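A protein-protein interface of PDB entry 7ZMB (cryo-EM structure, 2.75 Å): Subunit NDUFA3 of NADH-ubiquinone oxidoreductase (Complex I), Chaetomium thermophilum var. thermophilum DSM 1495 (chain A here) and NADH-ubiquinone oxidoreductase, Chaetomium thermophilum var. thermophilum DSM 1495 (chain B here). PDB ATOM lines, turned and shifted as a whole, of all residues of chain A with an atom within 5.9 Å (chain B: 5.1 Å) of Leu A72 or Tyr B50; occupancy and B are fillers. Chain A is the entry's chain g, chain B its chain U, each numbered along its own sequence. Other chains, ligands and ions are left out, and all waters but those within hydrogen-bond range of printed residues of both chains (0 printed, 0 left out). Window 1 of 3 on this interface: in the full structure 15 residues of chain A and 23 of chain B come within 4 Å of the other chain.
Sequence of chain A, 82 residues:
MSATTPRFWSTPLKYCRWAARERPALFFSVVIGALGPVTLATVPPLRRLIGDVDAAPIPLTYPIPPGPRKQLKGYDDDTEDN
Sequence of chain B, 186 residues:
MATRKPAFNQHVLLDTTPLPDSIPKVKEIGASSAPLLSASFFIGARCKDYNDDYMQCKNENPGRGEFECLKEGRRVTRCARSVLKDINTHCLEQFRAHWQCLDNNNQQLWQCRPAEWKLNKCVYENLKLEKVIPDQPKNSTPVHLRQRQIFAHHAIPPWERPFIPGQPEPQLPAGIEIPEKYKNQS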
ATOM      1  N   LYS A  70      26.359  19.276   5.496  1.00  0.00           N
ATOM      2  CA  LYS A  70      27.172  18.188   6.024  1.00  0.00           C
ATOM      3  C   LYS A  70      27.948  17.418   4.963  1.00  0.00           C
ATOM      4  O   LYS A  70      28.647  16.463   5.321  1.00  0.00           O
ATOM      5  CB  LYS A  70      26.292  17.222   6.821  1.00  0.00           C
ATOM      6  CG  LYS A  70      25.999  17.691   8.234  1.00  0.00           C
ATOM      7  CD  LYS A  70      24.784  16.991   8.818  1.00  0.00           C
ATOM      8  CE  LYS A  70      25.161  15.665   9.450  1.00  0.00           C
ATOM      9  NZ  LYS A  70      25.794  15.848  10.784  1.00  0.00           N
ATOM     10  N   GLN A  71      27.857  17.797   3.687  1.00  0.00           N
ATOM     11  CA  GLN A  71      28.620  17.154   2.614  1.00  0.00           C
ATOM     12  C   GLN A  71      28.313  15.655   2.557  1.00  0.00           C
ATOM     13  O   GLN A  71      29.152  14.794   2.818  1.00  0.00           O
ATOM     14  CB  GLN A  71      30.124  17.408   2.782  1.00  0.00           C
ATOM     15  CG  GLN A  71      30.671  18.504   1.886  1.00  0.00           C
ATOM     16  CD  GLN A  71      30.688  18.105   0.423  1.00  0.00           C
ATOM     17  OE1 GLN A  71      31.167  17.027   0.069  1.00  0.00           O
ATOM     18  NE2 GLN A  71      30.165  18.973  -0.434  1.00  0.00           N
ATOM     19  N   LEU A  72      27.064  15.376   2.206  1.00  0.00           N
ATOM     20  CA  LEU A  72      26.516  14.031   2.247  1.00  0.00           C
ATOM     21  C   LEU A  72      26.836  13.260   0.976  1.00  0.00           C
ATOM     22  O   LEU A  72      26.696  13.781  -0.134  1.00  0.00           O
ATOM     23  CB  LEU A  72      25.005  14.095   2.439  1.00  0.00           C
ATOM     24  CG  LEU A  72      24.553  14.663   3.775  1.00  0.00           C
ATOM     25  CD1 LEU A  72      23.072  14.810   3.763  1.00  0.00           C
ATOM     26  CD2 LEU A  72      24.973  13.733   4.887  1.00  0.00           C
ATOM     27  N   LYS A  73      27.262  12.013   1.148  1.00  0.00           N
ATOM     28  CA  LYS A  73      27.462  11.087   0.044  1.00  0.00           C
ATOM     29  C   LYS A  73      26.513   9.913   0.221  1.00  0.00           C
ATOM     30  O   LYS A  73      26.431   9.335   1.309  1.00  0.00           O
ATOM     31  CB  LYS A  73      28.910  10.597  -0.020  1.00  0.00           C
ATOM     32  CG  LYS A  73      29.937  11.713  -0.118  1.00  0.00           C
ATOM     33  CD  LYS A  73      31.281  11.185  -0.593  1.00  0.00           C
ATOM     34  CE  LYS A  73      31.710   9.961   0.199  1.00  0.00           C
ATOM     35  NZ  LYS A  73      31.811  10.249   1.656  1.00  0.00           N
ATOM     36  N   GLY A  74      25.756   9.587  -0.831  1.00  0.00           N
ATOM     37  CA  GLY A  74      24.752   8.510  -0.724  1.00  0.00           C
ATOM     38  C   GLY A  74      23.407   8.935  -1.271  1.00  0.00           C
ATOM     39  O   GLY A  74      23.126  10.136  -1.212  1.00  0.00           O
ATOM     40  N   TYR A  75      22.606   7.987  -1.763  1.00  0.00           N
ATOM     41  CA  TYR A  75      21.266   8.264  -2.354  1.00  0.00           C
ATOM     42  C   TYR A  75      21.390   9.143  -3.608  1.00  0.00           C
ATOM     43  O   TYR A  75      20.440   9.870  -3.938  1.00  0.00           O
ATOM     44  CB  TYR A  75      20.271   8.712  -1.285  1.00  0.00           C
ATOM     45  CG  TYR A  75      20.022   7.706  -0.192  1.00  0.00           C
ATOM     46  CD1 TYR A  75      19.318   6.540  -0.441  1.00  0.00           C
ATOM     47  CD2 TYR A  75      20.483   7.922   1.093  1.00  0.00           C
ATOM     48  CE1 TYR A  75      19.078   5.615   0.560  1.00  0.00           C
ATOM     49  CE2 TYR A  75      20.260   7.004   2.105  1.00  0.00           C
ATOM     50  CZ  TYR A  75      19.549   5.848   1.839  1.00  0.00           C
ATOM     51  OH  TYR A  75      19.323   4.939   2.832  1.00  0.00           O
ATOM     52  N   ASP A  76      22.483   9.001  -4.360  1.00  0.00           N
ATOM     53  CA  ASP A  76      22.682   9.864  -5.556  1.00  0.00           C
ATOM     54  C   ASP A  76      21.877   9.319  -6.745  1.00  0.00           C
ATOM     55  O   ASP A  76      21.207   8.297  -6.575  1.00  0.00           O
ATOM     56  CB  ASP A  76      24.169  10.033  -5.881  1.00  0.00           C
ATOM     57  CG  ASP A  76      24.904  10.892  -4.868  1.00  0.00           C
ATOM     58  OD1 ASP A  76      24.235  11.445  -3.972  1.00  0.00           O
ATOM     59  OD2 ASP A  76      26.141  11.002  -4.984  1.00  0.00           O
ATOM     60  N   ARG B  46      16.478   7.512   9.867  1.00  0.00           N
ATOM     61  CA  ARG B  46      17.462   7.207   8.796  1.00  0.00           C
ATOM     62  C   ARG B  46      17.767   8.393   7.869  1.00  0.00           C
ATOM     63  O   ARG B  46      18.953   8.556   7.523  1.00  0.00           O
ATOM     64  CB  ARG B  46      17.021   5.995   7.971  1.00  0.00           C
ATOM     65  CG  ARG B  46      17.839   5.803   6.702  1.00  0.00           C
ATOM     66  CD  ARG B  46      17.442   4.595   5.891  1.00  0.00           C
ATOM     67  NE  ARG B  46      17.533   3.378   6.673  1.00  0.00           N
ATOM     68  CZ  ARG B  46      16.992   2.231   6.297  1.00  0.00           C
ATOM     69  NH1 ARG B  46      17.107   1.155   7.052  1.00  0.00           N
ATOM     70  NH2 ARG B  46      16.326   2.171   5.162  1.00  0.00           N
ATOM     71  N   CYS B  47      16.780   9.220   7.502  1.00  0.00           N
ATOM     72  CA  CYS B  47      17.024  10.281   6.488  1.00  0.00           C
ATOM     73  C   CYS B  47      17.124  11.676   7.095  1.00  0.00           C
ATOM     74  O   CYS B  47      16.793  12.633   6.380  1.00  0.00           O
ATOM     75  CB  CYS B  47      15.892  10.288   5.474  1.00  0.00           C
ATOM     76  SG  CYS B  47      15.679   8.679   4.677  1.00  0.00           S
ATOM     77  N   LYS B  48      17.581  11.808   8.333  1.00  0.00           N
ATOM     78  CA  LYS B  48      17.580  13.166   8.921  1.00  0.00           C
ATOM     79  C   LYS B  48      18.564  14.029   8.142  1.00  0.00           C
ATOM     80  O   LYS B  48      18.198  15.154   7.811  1.00  0.00           O
ATOM     81  CB  LYS B  48      17.947  13.131  10.404  1.00  0.00           C
ATOM     82  CG  LYS B  48      17.610  14.396  11.179  1.00  0.00           C
ATOM     83  CD  LYS B  48      17.986  14.318  12.642  1.00  0.00           C
ATOM     84  CE  LYS B  48      19.462  14.063  12.859  1.00  0.00           C
ATOM     85  NZ  LYS B  48      19.793  13.953  14.299  1.00  0.00           N
ATOM     86  N   ASP B  49      19.745  13.500   7.840  1.00  0.00           N
ATOM     87  CA  ASP B  49      20.810  14.314   7.207  1.00  0.00           C
ATOM     88  C   ASP B  49      20.328  14.792   5.851  1.00  0.00           C
ATOM     89  O   ASP B  49      20.560  15.963   5.531  1.00  0.00           O
ATOM     90  CB  ASP B  49      22.082  13.482   7.063  1.00  0.00           C
ATOM     91  CG  ASP B  49      22.609  12.952   8.384  1.00  0.00           C
ATOM     92  OD1 ASP B  49      22.086  13.372   9.435  1.00  0.00           O
ATOM     93  OD2 ASP B  49      23.539  12.122   8.350  1.00  0.00           O
ATOM     94  N   TYR B  50      19.698  13.899   5.093  1.00  0.00           N
ATOM     95  CA  TYR B  50      19.189  14.234   3.742  1.00  0.00           C
ATOM     96  C   TYR B  50      18.041  15.230   3.860  1.00  0.00           C
ATOM     97  O   TYR B  50      18.032  16.215   3.112  1.00  0.00           O
ATOM     98  CB  TYR B  50      18.867  12.929   3.014  1.00  0.00           C
ATOM     99  CG  TYR B  50      20.030  11.970   3.008  1.00  0.00           C
ATOM    100  CD1 TYR B  50      20.200  11.032   4.012  1.00  0.00           C
ATOM    101  CD2 TYR B  50      20.998  12.042   2.021  1.00  0.00           C
ATOM    102  CE1 TYR B  50      21.284  10.171   4.019  1.00  0.00           C
ATOM    103  CE2 TYR B  50      22.084  11.186   2.011  1.00  0.00           C
ATOM    104  CZ  TYR B  50      22.229  10.247   3.012  1.00  0.00           C
ATOM    105  OH  TYR B  50      23.299   9.403   2.993  1.00  0.00           O
ATOM    106  N   ASN B  51      17.101  14.979   4.773  1.00  0.00           N
ATOM    107  CA  ASN B  51      15.987  15.930   5.026  1.00  0.00           C
ATOM    108  C   ASN B  51      16.586  17.270   5.437  1.00  0.00           C
ATOM    109  O   ASN B  51      16.161  18.300   4.887  1.00  0.00           O
ATOM    110  CB  ASN B  51      15.085  15.449   6.161  1.00  0.00           C
ATOM    111  CG  ASN B  51      14.234  14.254   5.794  1.00  0.00           C
ATOM    112  OD1 ASN B  51      14.256  13.796   4.654  1.00  0.00           O
ATOM    113  ND2 ASN B  51      13.475  13.744   6.750  1.00  0.00           N
ATOM    114  N   ASP B  52      17.556  17.249   6.348  1.00  0.00           N
ATOM    115  CA  ASP B  52      18.194  18.496   6.852  1.00  0.00           C
ATOM    116  C   ASP B  52      18.991  19.178   5.742  1.00  0.00           C
ATOM    117  O   ASP B  52      19.127  20.409   5.802  1.00  0.00           O
ATOM    118  CB  ASP B  52      19.006  18.237   8.118  1.00  0.00           C
ATOM    119  CG  ASP B  52      18.163  17.900   9.334  1.00  0.00           C
ATOM    120  OD1 ASP B  52      16.928  18.031   9.250  1.00  0.00           O
ATOM    121  OD2 ASP B  52      18.753  17.509  10.359  1.00  0.00           O
ATOM    122  N   ASP B  53      19.456  18.425   4.750  1.00  0.00           N
ATOM    123  CA  ASP B  53      20.322  18.995   3.687  1.00  0.00           C
ATOM    124  C   ASP B  53      19.429  19.697   2.667  1.00  0.00           C
ATOM    125  O   ASP B  53      19.806  20.789   2.219  1.00  0.00           O
ATOM    126  CB  ASP B  53      21.162  17.920   3.005  1.00  0.00           C
ATOM    127  CG  ASP B  53      22.367  18.462   2.261  1.00  0.00           C
ATOM    128  OD1 ASP B  53      22.956  19.444   2.743  1.00  0.00           O
ATOM    129  OD2 ASP B  53      22.703  17.893   1.205  1.00  0.00           O
ATOM    130  N   TYR B  54      18.311  19.066   2.306  1.00  0.00           N
ATOM    131  CA  TYR B  54      17.320  19.692   1.388  1.00  0.00           C
ATOM    132  C   TYR B  54      16.920  21.073   1.908  1.00  0.00           C
ATOM    133  O   TYR B  54      17.046  22.046   1.164  1.00  0.00           O
ATOM    134  CB  TYR B  54      16.165  18.727   1.113  1.00  0.00           C
ATOM    135  CG  TYR B  54      15.155  19.217   0.110  1.00  0.00           C
ATOM    136  CD1 TYR B  54      15.547  19.564  -1.168  1.00  0.00           C
ATOM    137  CD2 TYR B  54      13.816  19.332   0.436  1.00  0.00           C
ATOM    138  CE1 TYR B  54      14.635  20.016  -2.103  1.00  0.00           C
ATOM    139  CE2 TYR B  54      12.888  19.781  -0.488  1.00  0.00           C
ATOM    140  CZ  TYR B  54      13.303  20.123  -1.761  1.00  0.00           C
ATOM    141  OH  TYR B  54      12.419  20.572  -2.692  1.00  0.00           O
ATOM    142  N   GLU B  72      18.993  17.252  -4.077  1.00  0.00           N
ATOM    143  CA  GLU B  72      18.711  16.950  -2.652  1.00  0.00           C
ATOM    144  C   GLU B  72      17.310  16.349  -2.536  1.00  0.00           C
ATOM    145  O   GLU B  72      17.147  15.402  -1.767  1.00  0.00           O
ATOM    146  CB  GLU B  72      18.822  18.233  -1.829  1.00  0.00           C
ATOM    147  CG  GLU B  72      20.240  18.724  -1.608  1.00  0.00           C
ATOM    148  CD  GLU B  72      20.955  19.285  -2.825  1.00  0.00           C
ATOM    149  OE1 GLU B  72      20.271  19.711  -3.774  1.00  0.00           O
ATOM    150  OE2 GLU B  72      22.200  19.285  -2.820  1.00  0.00           O
ATOM    151  N   ARG B  75      17.325  12.895  -3.551  1.00  0.00           N
ATOM    152  CA  ARG B  75      18.031  12.142  -2.482  1.00  0.00           C
ATOM    153  C   ARG B  75      17.074  11.817  -1.320  1.00  0.00           C
ATOM    154  O   ARG B  75      17.140  10.692  -0.820  1.00  0.00           O
ATOM    155  CB  ARG B  75      19.236  12.976  -2.036  1.00  0.00           C
ATOM    156  CG  ARG B  75      20.481  12.184  -1.684  1.00  0.00           C
ATOM    157  CD  ARG B  75      21.653  13.080  -1.338  1.00  0.00           C
ATOM    158  NE  ARG B  75      21.979  14.048  -2.374  1.00  0.00           N
ATOM    159  CZ  ARG B  75      22.088  15.353  -2.161  1.00  0.00           C
ATOM    160  NH1 ARG B  75      22.391  16.163  -3.159  1.00  0.00           N
ATOM    161  NH2 ARG B  75      21.898  15.841  -0.948  1.00  0.00           N
ATOM    162  N   VAL B  76      16.227  12.764  -0.912  1.00  0.00           N
ATOM    163  CA  VAL B  76      15.242  12.512   0.190  1.00  0.00           C
ATOM    164  C   VAL B  76      14.218  11.472  -0.260  1.00  0.00           C
ATOM    165  O   VAL B  76      13.883  10.600   0.547  1.00  0.00           O
ATOM    166  CB  VAL B  76      14.589  13.784   0.782  1.00  0.00           C
ATOM    167  CG1 VAL B  76      15.620  14.845   1.117  1.00  0.00           C
ATOM    168  CG2 VAL B  76      13.483  14.364  -0.079  1.00  0.00           C
ATOM    169  N   CYS B  79      15.918   8.148  -0.196  1.00  0.00           N
ATOM    170  CA  CYS B  79      16.250   7.740   1.192  1.00  0.00           C
ATOM    171  C   CYS B  79      14.966   7.238   1.851  1.00  0.00           C
ATOM    172  O   CYS B  79      15.029   6.262   2.590  1.00  0.00           O
ATOM    173  CB  CYS B  79      16.867   8.910   1.943  1.00  0.00           C
ATOM    174  SG  CYS B  79      17.402   8.482   3.615  1.00  0.00           S
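OE2 of Glu B72 lies within salt-bridge range of NH1 of Arg B75 (3.1 Å). The side-chain sulfur (SG) of Cys B79 is disulfide-bonded to the side-chain sulfur (SG) of Cys B47. OD2 of Asp B53 lies within salt-bridge range of NH2 of Arg B75, at 3.1 Å.
Of the 13 printed residues of chain B, 6 touch a printed residue of chain A. Printed residues of chain A that touch a printed residue of chain B: Lys A70, Leu A72, Lys A73, Gly A74, Tyr A75 and Asp A76. Hydrophobic or aromatic side chains of chain A that line the printed part of chain B: Leu A72 and Tyr A75.
The side-chain carboxylate of Asp A76 lies within salt-bridge range of the guanidinium group of Arg B75 (3.8 Å).
Among the printed residues, pairs that only touch across the chains: Lys A70 with Asp B49 (3.8 Å), Leu A72 with Asp B49 (3.3 Å), Leu A72 with Tyr B50 (3.7 Å), Leu A72 with Asp B53 (3.7 Å), Lys A73 with Tyr B50 (3.6 Å), Gly A74 with Tyr B50 (3.5 Å), Gly A74 with Arg B75 (3.3 Å), Tyr A75 with Arg B46 (3.6 Å), Tyr A75 with Tyr B50 (3.5 Å), Tyr A75 with Arg B75 (3.2 Å) and Tyr A75 with Cys B79 (3.6 Å).
Printed residues of chain B within 4 Å of Leu A72: Asp B49 (3.3 Å), Tyr B50 (3.7 Å) and Asp B53 (3.7 Å). Of the printed residues of chain B, Gly A74 touches Tyr B50 and Arg B75. Lys B48 touches none of the printed residues of chain A. Tyr B50 touches just these residues of chain A: Leu A72, Lys A73, Gly A74 and Tyr A75. Printed residues of chain A within 4 Å of Arg B75: Gly A74 (3.3 Å), Tyr A75 (3.2 Å) and Asp A76 (3.8 Å). The nearest printed residue of chain A that does not touch Arg B75 is Leu A72 (4.9 Å).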
